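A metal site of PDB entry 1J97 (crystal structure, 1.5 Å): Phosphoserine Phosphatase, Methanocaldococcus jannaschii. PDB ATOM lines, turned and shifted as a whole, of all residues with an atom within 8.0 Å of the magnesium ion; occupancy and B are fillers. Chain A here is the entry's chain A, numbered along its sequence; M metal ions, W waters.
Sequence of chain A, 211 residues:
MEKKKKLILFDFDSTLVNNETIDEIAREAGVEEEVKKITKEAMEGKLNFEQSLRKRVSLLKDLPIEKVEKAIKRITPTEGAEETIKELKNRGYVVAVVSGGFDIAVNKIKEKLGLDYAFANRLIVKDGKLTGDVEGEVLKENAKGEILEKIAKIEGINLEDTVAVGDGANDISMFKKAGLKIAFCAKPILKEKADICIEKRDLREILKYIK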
ATOM      1  N   PHE A  10      -4.027  18.329 -15.407  1.00  0.00           N
ATOM      2  CA  PHE A  10      -3.543  19.693 -15.271  1.00  0.00           C
ATOM      3  C   PHE A  10      -2.157  19.829 -15.840  1.00  0.00           C
ATOM      4  O   PHE A  10      -1.276  18.973 -15.605  1.00  0.00           O
ATOM      5  CB  PHE A  10      -3.391  20.066 -13.787  1.00  0.00           C
ATOM      6  CG  PHE A  10      -4.681  20.235 -13.032  1.00  0.00           C
ATOM      7  CD1 PHE A  10      -5.307  21.482 -13.005  1.00  0.00           C
ATOM      8  CD2 PHE A  10      -5.265  19.166 -12.365  1.00  0.00           C
ATOM      9  CE1 PHE A  10      -6.496  21.667 -12.292  1.00  0.00           C
ATOM     10  CE2 PHE A  10      -6.471  19.340 -11.643  1.00  0.00           C
ATOM     11  CZ  PHE A  10      -7.068  20.587 -11.613  1.00  0.00           C
ATOM     12  N   BFD A  11      -1.930  20.928 -16.553  1.00  0.00           N
ATOM     13  CA  BFD A  11      -0.593  21.273 -16.964  1.00  0.00           C
ATOM     14  C   BFD A  11       0.087  21.798 -15.650  1.00  0.00           C
ATOM     15  O   BFD A  11      -0.570  22.199 -14.688  1.00  0.00           O
ATOM     16  CB  BFD A  11      -0.673  22.385 -18.028  1.00  0.00           C
ATOM     17  CG  BFD A  11       0.658  23.076 -18.262  1.00  0.00           C
ATOM     18  OD1 BFD A  11       1.638  22.361 -18.584  1.00  0.00           O
ATOM     19  OD2 BFD A  11       0.673  24.314 -18.046  1.00  0.00           O
ATOM     20 BE   BFD A  11       3.131  22.709 -18.679  1.00  0.00          BE
ATOM     21  F1  BFD A  11       3.675  21.992 -19.891  1.00  0.00           F
ATOM     22  F2  BFD A  11       3.421  24.185 -18.845  1.00  0.00           F
ATOM     23  F3  BFD A  11       3.807  22.204 -17.417  1.00  0.00           F
ATOM     24  N   PHE A  12       1.416  21.781 -15.611  1.00  0.00           N
ATOM     25  CA  PHE A  12       2.159  22.263 -14.464  1.00  0.00           C
ATOM     26  C   PHE A  12       2.568  23.751 -14.552  1.00  0.00           C
ATOM     27  O   PHE A  12       1.987  24.613 -13.870  1.00  0.00           O
ATOM     28  CB  PHE A  12       3.409  21.406 -14.275  1.00  0.00           C
ATOM     29  CG  PHE A  12       4.206  21.755 -13.052  1.00  0.00           C
ATOM     30  CD1 PHE A  12       3.704  21.480 -11.778  1.00  0.00           C
ATOM     31  CD2 PHE A  12       5.467  22.305 -13.172  1.00  0.00           C
ATOM     32  CE1 PHE A  12       4.475  21.772 -10.638  1.00  0.00           C
ATOM     33  CE2 PHE A  12       6.227  22.593 -12.024  1.00  0.00           C
ATOM     34  CZ  PHE A  12       5.723  22.320 -10.764  1.00  0.00           C
ATOM     35  N   ASP A  13       3.561  24.060 -15.394  1.00  0.00           N
ATOM     36  CA  ASP A  13       4.094  25.420 -15.496  1.00  0.00           C
ATOM     37  C   ASP A  13       3.060  26.432 -15.926  1.00  0.00           C
ATOM     38  O   ASP A  13       2.429  26.283 -16.965  1.00  0.00           O
ATOM     39  CB  ASP A  13       5.320  25.405 -16.437  1.00  0.00           C
ATOM     40  CG  ASP A  13       6.485  24.626 -15.844  1.00  0.00           C
ATOM     41  OD1 ASP A  13       6.892  23.584 -16.410  1.00  0.00           O
ATOM     42  OD2 ASP A  13       6.973  25.044 -14.769  1.00  0.00           O
ATOM     43  N   SER A  14       2.900  27.477 -15.106  1.00  0.00           N
ATOM     44  CA  SER A  14       1.946  28.564 -15.277  1.00  0.00           C
ATOM     45  C   SER A  14       0.490  28.126 -15.063  1.00  0.00           C
ATOM     46  O   SER A  14      -0.414  28.962 -15.131  1.00  0.00           O
ATOM     47  CB  SER A  14       2.101  29.296 -16.642  1.00  0.00           C
ATOM     48  OG  SER A  14       3.382  29.950 -16.679  1.00  0.00           O
ATOM     49  N   THR A  15       0.246  26.839 -14.755  1.00  0.00           N
ATOM     50  CA  THR A  15      -1.139  26.376 -14.483  1.00  0.00           C
ATOM     51  C   THR A  15      -1.224  25.933 -13.010  1.00  0.00           C
ATOM     52  O   THR A  15      -1.788  26.671 -12.203  1.00  0.00           O
ATOM     53  CB  THR A  15      -1.566  25.248 -15.482  1.00  0.00           C
ATOM     54  OG1 THR A  15      -1.643  25.812 -16.800  1.00  0.00           O
ATOM     55  CG2 THR A  15      -2.965  24.730 -15.179  1.00  0.00           C
ATOM     56  N   LEU A  16      -0.676  24.771 -12.632  1.00  0.00           N
ATOM     57  CA  LEU A  16      -0.679  24.362 -11.231  1.00  0.00           C
ATOM     58  C   LEU A  16       0.203  25.259 -10.372  1.00  0.00           C
ATOM     59  O   LEU A  16      -0.012  25.388  -9.164  1.00  0.00           O
ATOM     60  CB  LEU A  16      -0.205  22.928 -11.067  1.00  0.00           C
ATOM     61  CG  LEU A  16      -1.294  21.892 -11.304  1.00  0.00           C
ATOM     62  CD1 LEU A  16      -0.653  20.523 -11.219  1.00  0.00           C
ATOM     63  CD2 LEU A  16      -2.403  21.989 -10.210  1.00  0.00           C
ATOM     64  N   VAL A  17       1.257  25.812 -10.981  1.00  0.00           N
ATOM     65  CA  VAL A  17       2.135  26.728 -10.277  1.00  0.00           C
ATOM     66  C   VAL A  17       2.160  28.041 -11.019  1.00  0.00           C
ATOM     67  O   VAL A  17       1.825  28.110 -12.215  1.00  0.00           O
ATOM     68  CB  VAL A  17       3.589  26.159 -10.107  1.00  0.00           C
ATOM     69  CG1 VAL A  17       3.538  24.896  -9.269  1.00  0.00           C
ATOM     70  CG2 VAL A  17       4.182  25.846 -11.466  1.00  0.00           C
ATOM     71  N   ASN A  19       4.768  29.909 -11.795  1.00  0.00           N
ATOM     72  CA  ASN A  19       6.019  30.102 -12.517  1.00  0.00           C
ATOM     73  C   ASN A  19       6.263  29.199 -13.697  1.00  0.00           C
ATOM     74  O   ASN A  19       5.538  28.235 -13.918  1.00  0.00           O
ATOM     75  CB  ASN A  19       7.222  29.818 -11.589  1.00  0.00           C
ATOM     76  CG  ASN A  19       7.007  30.149 -10.123  1.00  0.00           C
ATOM     77  OD1 ASN A  19       6.120  29.606  -9.435  1.00  0.00           O
ATOM     78  ND2 ASN A  19       7.883  31.000  -9.607  1.00  0.00           N
ATOM     79  N   GLU A  20       7.324  29.513 -14.411  1.00  0.00           N
ATOM     80  CA  GLU A  20       7.820  28.689 -15.502  1.00  0.00           C
ATOM     81  C   GLU A  20       9.130  28.130 -14.950  1.00  0.00           C
ATOM     82  O   GLU A  20      10.120  28.875 -14.775  1.00  0.00           O
ATOM     83  CB  GLU A  20       8.081  29.487 -16.772  1.00  0.00           C
ATOM     84  CG  GLU A  20       6.812  29.872 -17.526  1.00  0.00           C
ATOM     85  CD  GLU A  20       6.154  28.671 -18.220  1.00  0.00           C
ATOM     86  OE1 GLU A  20       6.864  27.688 -18.519  1.00  0.00           O
ATOM     87  OE2 GLU A  20       4.934  28.751 -18.475  1.00  0.00           O
ATOM     88  N   THR A  39      10.588  30.811 -24.193  1.00  0.00           N
ATOM     89  CA  THR A  39       9.458  30.206 -23.501  1.00  0.00           C
ATOM     90  C   THR A  39       8.156  30.867 -23.903  1.00  0.00           C
ATOM     91  O   THR A  39       7.157  30.198 -24.189  1.00  0.00           O
ATOM     92  CB  THR A  39       9.652  30.322 -21.964  1.00  0.00           C
ATOM     93  OG1 THR A  39      10.820  29.581 -21.604  1.00  0.00           O
ATOM     94  CG2 THR A  39       8.423  29.768 -21.200  1.00  0.00           C
ATOM     95  N   MET A  43       5.085  28.971 -25.788  1.00  0.00           N
ATOM     96  CA  MET A  43       3.746  28.874 -25.214  1.00  0.00           C
ATOM     97  C   MET A  43       2.704  29.622 -26.045  1.00  0.00           C
ATOM     98  O   MET A  43       1.525  29.296 -25.985  1.00  0.00           O
ATOM     99  CB  MET A  43       3.754  29.299 -23.752  1.00  0.00           C
ATOM    100  CG  MET A  43       4.554  28.310 -22.847  1.00  0.00           C
ATOM    101  SD  MET A  43       3.917  26.543 -22.865  1.00  0.00           S
ATOM    102  CE  MET A  43       4.946  25.881 -24.139  1.00  0.00           C
ATOM    103  N   VAL A  98       0.493  16.765 -16.221  1.00  0.00           N
ATOM    104  CA  VAL A  98       1.196  16.432 -17.468  1.00  0.00           C
ATOM    105  C   VAL A  98       1.886  17.715 -17.891  1.00  0.00           C
ATOM    106  O   VAL A  98       1.216  18.717 -18.208  1.00  0.00           O
ATOM    107  CB  VAL A  98       0.213  15.968 -18.551  1.00  0.00           C
ATOM    108  CG1 VAL A  98       0.954  15.518 -19.798  1.00  0.00           C
ATOM    109  CG2 VAL A  98      -0.644  14.812 -17.979  1.00  0.00           C
ATOM    110  N   SER A  99       3.213  17.659 -17.944  1.00  0.00           N
ATOM    111  CA  SER A  99       4.059  18.826 -18.153  1.00  0.00           C
ATOM    112  C   SER A  99       5.196  18.648 -19.125  1.00  0.00           C
ATOM    113  O   SER A  99       5.860  17.598 -19.138  1.00  0.00           O
ATOM    114  CB  SER A  99       4.675  19.151 -16.792  1.00  0.00           C
ATOM    115  OG  SER A  99       5.540  20.286 -16.856  1.00  0.00           O
ATOM    116  N   GLY A 100       5.438  19.707 -19.896  1.00  0.00           N
ATOM    117  CA  GLY A 100       6.587  19.764 -20.787  1.00  0.00           C
ATOM    118  C   GLY A 100       7.829  20.179 -20.001  1.00  0.00           C
ATOM    119  O   GLY A 100       8.905  20.343 -20.579  1.00  0.00           O
ATOM    120  N   GLY A 101       7.673  20.320 -18.684  1.00  0.00           N
ATOM    121  CA  GLY A 101       8.734  20.671 -17.765  1.00  0.00           C
ATOM    122  C   GLY A 101       9.530  19.484 -17.253  1.00  0.00           C
ATOM    123  O   GLY A 101       9.691  18.478 -17.945  1.00  0.00           O
ATOM    124  N   LYS A 144       0.908  15.343 -25.054  1.00  0.00           N
ATOM    125  CA  LYS A 144      -0.066  15.328 -23.987  1.00  0.00           C
ATOM    126  C   LYS A 144      -1.354  14.613 -24.347  1.00  0.00           C
ATOM    127  O   LYS A 144      -1.968  13.994 -23.478  1.00  0.00           O
ATOM    128  CB  LYS A 144      -0.346  16.744 -23.468  1.00  0.00           C
ATOM    129  CG  LYS A 144       0.908  17.421 -22.915  1.00  0.00           C
ATOM    130  CD  LYS A 144       0.530  18.572 -22.035  1.00  0.00           C
ATOM    131  CE  LYS A 144       1.813  19.345 -21.632  1.00  0.00           C
ATOM    132  NZ  LYS A 144       1.504  20.446 -20.647  1.00  0.00           N
ATOM    133  N   VAL A 165      -6.854  21.061 -18.361  1.00  0.00           N
ATOM    134  CA  VAL A 165      -6.666  22.439 -17.834  1.00  0.00           C
ATOM    135  C   VAL A 165      -5.227  22.866 -18.112  1.00  0.00           C
ATOM    136  O   VAL A 165      -4.280  22.247 -17.603  1.00  0.00           O
ATOM    137  CB  VAL A 165      -6.907  22.480 -16.310  1.00  0.00           C
ATOM    138  CG1 VAL A 165      -6.872  23.918 -15.826  1.00  0.00           C
ATOM    139  CG2 VAL A 165      -8.258  21.876 -15.932  1.00  0.00           C
ATOM    140  N   GLY A 166      -5.040  23.934 -18.903  1.00  0.00           N
ATOM    141  CA  GLY A 166      -3.702  24.386 -19.242  1.00  0.00           C
ATOM    142  C   GLY A 166      -3.673  25.832 -19.656  1.00  0.00           C
ATOM    143  O   GLY A 166      -4.712  26.507 -19.705  1.00  0.00           O
ATOM    144  N   ASP A 167      -2.477  26.320 -19.985  1.00  0.00           N
ATOM    145  CA  ASP A 167      -2.291  27.716 -20.335  1.00  0.00           C
ATOM    146  C   ASP A 167      -1.584  27.937 -21.653  1.00  0.00           C
ATOM    147  O   ASP A 167      -1.706  29.032 -22.223  1.00  0.00           O
ATOM    148  CB  ASP A 167      -1.405  28.433 -19.284  1.00  0.00           C
ATOM    149  CG  ASP A 167       0.039  27.969 -19.358  1.00  0.00           C
ATOM    150  OD1 ASP A 167       0.280  26.818 -18.957  1.00  0.00           O
ATOM    151  OD2 ASP A 167       0.938  28.692 -19.858  1.00  0.00           O
ATOM    152  N   GLY A 168      -0.863  26.930 -22.151  1.00  0.00           N
ATOM    153  CA  GLY A 168      -0.012  27.114 -23.307  1.00  0.00           C
ATOM    154  C   GLY A 168      -0.239  26.265 -24.528  1.00  0.00           C
ATOM    155  O   GLY A 168      -1.028  25.346 -24.524  1.00  0.00           O
ATOM    156  N   ALA A 169       0.510  26.583 -25.579  1.00  0.00           N
ATOM    157  CA  ALA A 169       0.356  25.843 -26.824  1.00  0.00           C
ATOM    158  C   ALA A 169       0.613  24.352 -26.730  1.00  0.00           C
ATOM    159  O   ALA A 169       0.072  23.588 -27.542  1.00  0.00           O
ATOM    160  CB  ALA A 169       1.231  26.453 -27.898  1.00  0.00           C
ATOM    161  N   ASN A 170       1.431  23.906 -25.762  1.00  0.00           N
ATOM    162  CA  ASN A 170       1.710  22.489 -25.654  1.00  0.00           C
ATOM    163  C   ASN A 170       0.572  21.715 -24.961  1.00  0.00           C
ATOM    164  O   ASN A 170       0.664  20.485 -24.802  1.00  0.00           O
ATOM    165  CB  ASN A 170       3.091  22.245 -25.005  1.00  0.00           C
ATOM    166  CG  ASN A 170       3.162  22.680 -23.566  1.00  0.00           C
ATOM    167  OD1 ASN A 170       2.499  23.620 -23.164  1.00  0.00           O
ATOM    168  ND2 ASN A 170       3.975  22.008 -22.785  1.00  0.00           N
ATOM    169  N   ASP A 171      -0.489  22.437 -24.597  1.00  0.00           N
ATOM    170  CA  ASP A 171      -1.713  21.851 -24.033  1.00  0.00           C
ATOM    171  C   ASP A 171      -2.766  21.602 -25.127  1.00  0.00           C
ATOM    172  O   ASP A 171      -3.775  20.954 -24.897  1.00  0.00           O
ATOM    173  CB  ASP A 171      -2.252  22.782 -22.915  1.00  0.00           C
ATOM    174  CG  ASP A 171      -1.265  22.915 -21.777  1.00  0.00           C
ATOM    175  OD1 ASP A 171      -0.719  21.865 -21.428  1.00  0.00           O
ATOM    176  OD2 ASP A 171      -1.009  24.053 -21.264  1.00  0.00           O
ATOM    177  N   PHE A 184      -6.687  28.167 -18.630  1.00  0.00           N
ATOM    178  CA  PHE A 184      -6.487  28.892 -17.379  1.00  0.00           C
ATOM    179  C   PHE A 184      -5.493  30.044 -17.532  1.00  0.00           C
ATOM    180  O   PHE A 184      -4.300  29.785 -17.679  1.00  0.00           O
ATOM    181  CB  PHE A 184      -5.977  27.900 -16.339  1.00  0.00           C
ATOM    182  CG  PHE A 184      -5.849  28.500 -14.958  1.00  0.00           C
ATOM    183  CD1 PHE A 184      -6.984  28.812 -14.192  1.00  0.00           C
ATOM    184  CD2 PHE A 184      -4.594  28.768 -14.424  1.00  0.00           C
ATOM    185  CE1 PHE A 184      -6.850  29.393 -12.907  1.00  0.00           C
ATOM    186  CE2 PHE A 184      -4.447  29.350 -13.170  1.00  0.00           C
ATOM    187  CZ  PHE A 184      -5.589  29.656 -12.404  1.00  0.00           C
ATOM    188  N   LEU A 190      -4.354  29.029 -27.084  1.00  0.00           N
ATOM    189  CA  LEU A 190      -5.091  27.979 -26.392  1.00  0.00           C
ATOM    190  C   LEU A 190      -6.510  28.487 -26.121  1.00  0.00           C
ATOM    191  O   LEU A 190      -7.490  27.718 -26.207  1.00  0.00           O
ATOM    192  CB  LEU A 190      -4.366  27.564 -25.075  1.00  0.00           C
ATOM    193  CG  LEU A 190      -4.944  26.326 -24.388  1.00  0.00           C
ATOM    194  CD1 LEU A 190      -4.622  25.036 -25.184  1.00  0.00           C
ATOM    195  CD2 LEU A 190      -4.373  26.215 -22.971  1.00  0.00           C
HETATM  196 MG    MG M   1       2.005  25.632 -18.902  1.00  0.00          MG
HETATM  197  O   HOH W   1       3.094  27.201 -19.704  1.00  0.00           O
HETATM  198  O   HOH W   2       1.471  24.877 -20.823  1.00  0.00           O
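N of BFD 11 lies within hydrogen-bond range of the backbone carbonyl oxygen (O) of Val 165, at 2.9 Å. N of Leu 16 sits at hydrogen-bond distance from O of BFD 11, 3.3 Å away. OD1 of BFD 11 lies within salt-bridge range of NZ of Lys 144 (2.8 Å). The side-chain carboxylate (OD2) of Asp 171 sits at hydrogen-bond distance from the backbone NH (N) of Asp 167, 3.0 Å away. OD2 of BFD 11 sits close to the side-chain hydroxyl (OG1) of Thr 15 (3.0 Å). The side-chain hydroxyl of Thr 15 lies within hydrogen-bond range of the backbone NH of Asp 167 (3.3 Å).
The nearest printed residue that does not touch the magnesium ion is Asp 171 (4.1 Å).
F2 of BFD 11 binds the magnesium ion. OD2 of BFD 11 binds the magnesium ion (2.1 Å). Water W1 binds the magnesium ion (2.1 Å). The magnesium ion is bound by O of Asp 13 (2.1 Å). The side-chain carboxylate (OD1) of Asp 167 is bound to the magnesium ion (2.1 Å). Water W2 is bound to the magnesium ion (2.1 Å).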
